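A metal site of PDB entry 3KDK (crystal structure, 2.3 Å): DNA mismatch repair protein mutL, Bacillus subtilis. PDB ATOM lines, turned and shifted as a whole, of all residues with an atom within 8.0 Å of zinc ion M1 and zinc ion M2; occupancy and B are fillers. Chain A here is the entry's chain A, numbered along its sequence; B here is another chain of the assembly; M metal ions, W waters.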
ATOM      1  N   ASP A  32       7.689  21.405  -8.865  1.00  0.00           N
ATOM      2  CA  ASP A  32       6.385  21.828  -9.334  1.00  0.00           C
ATOM      3  C   ASP A  32       6.050  21.008 -10.568  1.00  0.00           C
ATOM      4  O   ASP A  32       6.637  21.208 -11.637  1.00  0.00           O
ATOM      5  CB  ASP A  32       6.401  23.323  -9.667  1.00  0.00           C
ATOM      6  CG  ASP A  32       5.018  23.865  -9.980  1.00  0.00           C
ATOM      7  OD1 ASP A  32       4.421  23.410 -10.973  1.00  0.00           O
ATOM      8  OD2 ASP A  32       4.532  24.726  -9.220  1.00  0.00           O
ATOM      9  N   HIS A  34       3.466  20.700 -12.575  1.00  0.00           N
ATOM     10  CA  HIS A  34       2.890  21.371 -13.731  1.00  0.00           C
ATOM     11  C   HIS A  34       3.942  22.162 -14.512  1.00  0.00           C
ATOM     12  O   HIS A  34       4.001  22.075 -15.744  1.00  0.00           O
ATOM     13  CB  HIS A  34       1.754  22.308 -13.334  1.00  0.00           C
ATOM     14  CG  HIS A  34       1.097  22.966 -14.508  1.00  0.00           C
ATOM     15  ND1 HIS A  34       0.029  22.408 -15.166  1.00  0.00           N
ATOM     16  CD2 HIS A  34       1.399  24.105 -15.160  1.00  0.00           C
ATOM     17  CE1 HIS A  34      -0.323  23.194 -16.168  1.00  0.00           C
ATOM     18  NE2 HIS A  34       0.490  24.233 -16.187  1.00  0.00           N
ATOM     19  N   ALA A  35       4.753  22.939 -13.806  1.00  0.00           N
ATOM     20  CA  ALA A  35       5.850  23.675 -14.424  1.00  0.00           C
ATOM     21  C   ALA A  35       6.782  22.719 -15.159  1.00  0.00           C
ATOM     22  O   ALA A  35       7.288  23.029 -16.246  1.00  0.00           O
ATOM     23  CB  ALA A  35       6.621  24.475 -13.374  1.00  0.00           C
ATOM     24  N   ALA A  36       7.017  21.550 -14.554  1.00  0.00           N
ATOM     25  CA  ALA A  36       7.875  20.526 -15.163  1.00  0.00           C
ATOM     26  C   ALA A  36       7.268  20.033 -16.463  1.00  0.00           C
ATOM     27  O   ALA A  36       7.953  19.956 -17.487  1.00  0.00           O
ATOM     28  CB  ALA A  36       8.080  19.361 -14.203  1.00  0.00           C
ATOM     29  N   GLN A  37       5.990  19.699 -16.428  1.00  0.00           N
ATOM     30  CA  GLN A  37       5.276  19.220 -17.614  1.00  0.00           C
ATOM     31  C   GLN A  37       5.292  20.266 -18.744  1.00  0.00           C
ATOM     32  O   GLN A  37       5.392  19.904 -19.918  1.00  0.00           O
ATOM     33  CB  GLN A  37       3.845  18.818 -17.248  1.00  0.00           C
ATOM     34  CG  GLN A  37       3.777  17.596 -16.337  1.00  0.00           C
ATOM     35  CD  GLN A  37       2.416  17.420 -15.684  1.00  0.00           C
ATOM     36  OE1 GLN A  37       1.617  18.348 -15.608  1.00  0.00           O
ATOM     37  NE2 GLN A  37       2.143  16.205 -15.199  1.00  0.00           N
ATOM     38  N   GLU A  38       5.217  21.543 -18.381  1.00  0.00           N
ATOM     39  CA  GLU A  38       5.329  22.627 -19.356  1.00  0.00           C
ATOM     40  C   GLU A  38       6.667  22.616 -20.076  1.00  0.00           C
ATOM     41  O   GLU A  38       6.736  22.687 -21.304  1.00  0.00           O
ATOM     42  CB  GLU A  38       5.175  23.988 -18.667  1.00  0.00           C
ATOM     43  CG  GLU A  38       3.786  24.372 -18.244  1.00  0.00           C
ATOM     44  CD  GLU A  38       3.733  25.815 -17.786  1.00  0.00           C
ATOM     45  OE1 GLU A  38       2.632  26.316 -17.468  1.00  0.00           O
ATOM     46  OE2 GLU A  38       4.803  26.456 -17.758  1.00  0.00           O
ATOM     47  N   ARG A  39       7.747  22.569 -19.295  1.00  0.00           N
ATOM     48  CA  ARG A  39       9.093  22.564 -19.853  1.00  0.00           C
ATOM     49  C   ARG A  39       9.254  21.405 -20.823  1.00  0.00           C
ATOM     50  O   ARG A  39       9.712  21.587 -21.955  1.00  0.00           O
ATOM     51  CB  ARG A  39      10.135  22.455 -18.729  1.00  0.00           C
ATOM     52  CG  ARG A  39      11.488  21.990 -19.228  1.00  0.00           C
ATOM     53  CD  ARG A  39      12.051  22.923 -20.289  1.00  0.00           C
ATOM     54  NE  ARG A  39      12.110  24.297 -19.817  1.00  0.00           N
ATOM     55  CZ  ARG A  39      12.459  25.332 -20.580  1.00  0.00           C
ATOM     56  NH1 ARG A  39      12.799  25.148 -21.841  1.00  0.00           N
ATOM     57  NH2 ARG A  39      12.484  26.561 -20.062  1.00  0.00           N
ATOM     58  N   ILE A 139       4.771  27.198 -27.055  1.00  0.00           N
ATOM     59  CA  ILE A 139       4.257  27.475 -25.724  1.00  0.00           C
ATOM     60  C   ILE A 139       2.775  27.124 -25.619  1.00  0.00           C
ATOM     61  O   ILE A 139       2.333  26.503 -24.645  1.00  0.00           O
ATOM     62  CB  ILE A 139       4.430  28.963 -25.356  1.00  0.00           C
ATOM     63  CG1 ILE A 139       5.906  29.283 -25.128  1.00  0.00           C
ATOM     64  CG2 ILE A 139       3.616  29.300 -24.116  1.00  0.00           C
ATOM     65  CD1 ILE A 139       6.178  30.742 -24.802  1.00  0.00           C
ATOM     66  N   SER A 142       2.050  23.415 -25.274  1.00  0.00           N
ATOM     67  CA  SER A 142       2.559  22.759 -24.073  1.00  0.00           C
ATOM     68  C   SER A 142       1.597  22.878 -22.893  1.00  0.00           C
ATOM     69  O   SER A 142       1.596  22.043 -21.987  1.00  0.00           O
ATOM     70  CB  SER A 142       3.933  23.308 -23.703  1.00  0.00           C
ATOM     71  OG  SER A 142       3.905  24.718 -23.609  1.00  0.00           O
ATOM     72  N   CYS A 143       0.765  23.922 -22.895  1.00  0.00           N
ATOM     73  CA  CYS A 143      -0.277  24.080 -21.891  1.00  0.00           C
ATOM     74  C   CYS A 143      -1.589  23.569 -22.451  1.00  0.00           C
ATOM     75  O   CYS A 143      -2.643  23.723 -21.836  1.00  0.00           O
ATOM     76  CB  CYS A 143      -0.404  25.543 -21.480  1.00  0.00           C
ATOM     77  SG  CYS A 143       1.098  26.230 -20.750  1.00  0.00           S
ATOM     78  N   LYS A 144      -1.518  22.966 -23.631  1.00  0.00           N
ATOM     79  CA  LYS A 144      -2.683  22.446 -24.328  1.00  0.00           C
ATOM     80  C   LYS A 144      -2.833  20.941 -24.088  1.00  0.00           C
ATOM     81  O   LYS A 144      -3.195  20.508 -22.998  1.00  0.00           O
ATOM     82  CB  LYS A 144      -2.576  22.723 -25.825  1.00  0.00           C
ATOM     83  CG  LYS A 144      -3.898  23.048 -26.502  1.00  0.00           C
ATOM     84  CD  LYS A 144      -4.021  24.543 -26.803  1.00  0.00           C
ATOM     85  CE  LYS A 144      -3.943  25.373 -25.540  1.00  0.00           C
ATOM     86  NZ  LYS A 144      -3.930  26.834 -25.825  1.00  0.00           N
ATOM     87  N   THR A 173      13.807  25.912 -14.836  1.00  0.00           N
ATOM     88  CA  THR A 173      12.942  27.043 -15.149  1.00  0.00           C
ATOM     89  C   THR A 173      11.979  26.681 -16.265  1.00  0.00           C
ATOM     90  O   THR A 173      12.376  26.051 -17.247  1.00  0.00           O
ATOM     91  CB  THR A 173      13.799  28.277 -15.558  1.00  0.00           C
ATOM     92  OG1 THR A 173      14.795  28.526 -14.557  1.00  0.00           O
ATOM     93  CG2 THR A 173      12.934  29.509 -15.737  1.00  0.00           C
ATOM     94  N   CYS A 174      10.704  27.053 -16.115  1.00  0.00           N
ATOM     95  CA  CYS A 174       9.722  26.803 -17.165  1.00  0.00           C
ATOM     96  C   CYS A 174       9.783  27.895 -18.238  1.00  0.00           C
ATOM     97  O   CYS A 174      10.392  28.943 -18.017  1.00  0.00           O
ATOM     98  CB  CYS A 174       8.307  26.692 -16.586  1.00  0.00           C
ATOM     99  SG  CYS A 174       7.549  28.287 -16.255  1.00  0.00           S
ATOM    100  N   PRO A 175       9.159  27.640 -19.408  1.00  0.00           N
ATOM    101  CA  PRO A 175       9.252  28.584 -20.532  1.00  0.00           C
ATOM    102  C   PRO A 175       8.701  29.969 -20.195  1.00  0.00           C
ATOM    103  O   PRO A 175       8.911  30.909 -20.950  1.00  0.00           O
ATOM    104  CB  PRO A 175       8.390  27.921 -21.604  1.00  0.00           C
ATOM    105  CG  PRO A 175       8.359  26.473 -21.234  1.00  0.00           C
ATOM    106  CD  PRO A 175       8.364  26.456 -19.736  1.00  0.00           C
ATOM    107  N   HIS A 176       8.006  30.080 -19.065  1.00  0.00           N
ATOM    108  CA  HIS A 176       7.466  31.358 -18.630  1.00  0.00           C
ATOM    109  C   HIS A 176       8.372  32.068 -17.623  1.00  0.00           C
ATOM    110  O   HIS A 176       8.086  33.192 -17.207  1.00  0.00           O
ATOM    111  CB  HIS A 176       6.060  31.182 -18.046  1.00  0.00           C
ATOM    112  CG  HIS A 176       5.092  30.533 -18.987  1.00  0.00           C
ATOM    113  ND1 HIS A 176       4.897  29.174 -19.037  1.00  0.00           N
ATOM    114  CD2 HIS A 176       4.262  31.064 -19.920  1.00  0.00           C
ATOM    115  CE1 HIS A 176       3.990  28.886 -19.946  1.00  0.00           C
ATOM    116  NE2 HIS A 176       3.594  30.019 -20.506  1.00  0.00           N
ATOM    117  N   GLY A 177       9.462  31.423 -17.228  1.00  0.00           N
ATOM    118  CA  GLY A 177      10.434  32.036 -16.340  1.00  0.00           C
ATOM    119  C   GLY A 177      10.323  31.644 -14.872  1.00  0.00           C
ATOM    120  O   GLY A 177      11.145  32.047 -14.056  1.00  0.00           O
ATOM    121  N   ARG A 178       9.299  30.868 -14.538  1.00  0.00           N
ATOM    122  CA  ARG A 178       9.079  30.431 -13.165  1.00  0.00           C
ATOM    123  C   ARG A 178       9.879  29.177 -12.803  1.00  0.00           C
ATOM    124  O   ARG A 178      10.123  28.322 -13.645  1.00  0.00           O
ATOM    125  CB  ARG A 178       7.582  30.204 -12.906  1.00  0.00           C
ATOM    126  CG  ARG A 178       6.819  31.495 -12.668  1.00  0.00           C
ATOM    127  CD  ARG A 178       5.317  31.343 -12.840  1.00  0.00           C
ATOM    128  NE  ARG A 178       4.767  32.469 -13.581  1.00  0.00           N
ATOM    129  CZ  ARG A 178       4.212  32.374 -14.785  1.00  0.00           C
ATOM    130  NH1 ARG A 178       3.742  33.458 -15.398  1.00  0.00           N
ATOM    131  NH2 ARG A 178       4.105  31.190 -15.385  1.00  0.00           N
ATOM    132  N   PRO A 179      10.309  29.082 -11.528  1.00  0.00           N
ATOM    133  CA  PRO A 179      11.142  27.974 -11.060  1.00  0.00           C
ATOM    134  C   PRO A 179      10.404  26.650 -11.156  1.00  0.00           C
ATOM    135  O   PRO A 179       9.230  26.583 -10.821  1.00  0.00           O
ATOM    136  CB  PRO A 179      11.396  28.321  -9.581  1.00  0.00           C
ATOM    137  CG  PRO A 179      11.118  29.783  -9.481  1.00  0.00           C
ATOM    138  CD  PRO A 179      10.013  30.043 -10.456  1.00  0.00           C
ATOM    139  N   ILE A 180      11.090  25.608 -11.624  1.00  0.00           N
ATOM    140  CA  ILE A 180      10.543  24.260 -11.666  1.00  0.00           C
ATOM    141  C   ILE A 180      11.035  23.450 -10.456  1.00  0.00           C
ATOM    142  O   ILE A 180      10.307  22.616  -9.914  1.00  0.00           O
ATOM    143  CB  ILE A 180      10.964  23.511 -12.942  1.00  0.00           C
ATOM    144  CG1 ILE A 180      10.342  24.166 -14.179  1.00  0.00           C
ATOM    145  CG2 ILE A 180      10.534  22.044 -12.866  1.00  0.00           C
ATOM    146  CD1 ILE A 180      10.846  23.595 -15.479  1.00  0.00           C
ATOM    147  N   PHE B 193       7.798  29.092  -5.832  1.00  0.00           N
ATOM    148  CA  PHE B 193       7.643  28.678  -7.232  1.00  0.00           C
ATOM    149  C   PHE B 193       7.058  29.736  -8.172  1.00  0.00           C
ATOM    150  O   PHE B 193       7.001  29.508  -9.382  1.00  0.00           O
ATOM    151  CB  PHE B 193       6.813  27.401  -7.327  1.00  0.00           C
ATOM    152  CG  PHE B 193       7.531  26.172  -6.866  1.00  0.00           C
ATOM    153  CD1 PHE B 193       8.455  25.538  -7.689  1.00  0.00           C
ATOM    154  CD2 PHE B 193       7.278  25.627  -5.616  1.00  0.00           C
ATOM    155  CE1 PHE B 193       9.121  24.398  -7.267  1.00  0.00           C
ATOM    156  CE2 PHE B 193       7.938  24.482  -5.187  1.00  0.00           C
ATOM    157  CZ  PHE B 193       8.859  23.872  -6.010  1.00  0.00           C
HETATM  158 ZN    ZN M   1       5.114  28.389 -16.705  1.00  0.00          ZN
HETATM  159 ZN    ZN M   2       0.499  25.830 -17.912  1.00  0.00          ZN
HETATM  160  O   HOH W   1       3.025  28.820 -15.594  1.00  0.00           O
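OD1 of Asp 32 lies close to N of His 34. The side-chain sulfur of Cys 174 sits close to the backbone NH of Arg 178, 3.6 Å away. The side-chain carboxylate (OE1) of Glu 38 lies close to the side-chain sulfur (SG) of Cys 143 (3.6 Å).
Merely in contact with zinc ion M1: Arg 178 (3.3 Å).
Zinc ion M2 is bound by the side-chain carboxylate of Glu 38 (2.2 Å) and a ring nitrogen (NE2) of His 34 (2.4 Å). Slightly farther from zinc ion M2 lies SG of Cys 143 (2.9 Å).
Within 4 Å of zinc ion M2: His 34, Glu 38 and Cys 143. The nearest printed residue that does not touch zinc ion M2 is His 176 (5.1 Å).
OE2 of Glu 38 binds zinc ion M1. Water W1 is bound to zinc ion M1 (2.4 Å). Zinc ion M1 is bound by ND1 of His 176 (2.5 Å). Zinc ion M1 is bound by SG of Cys 174, 2.5 Å away.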
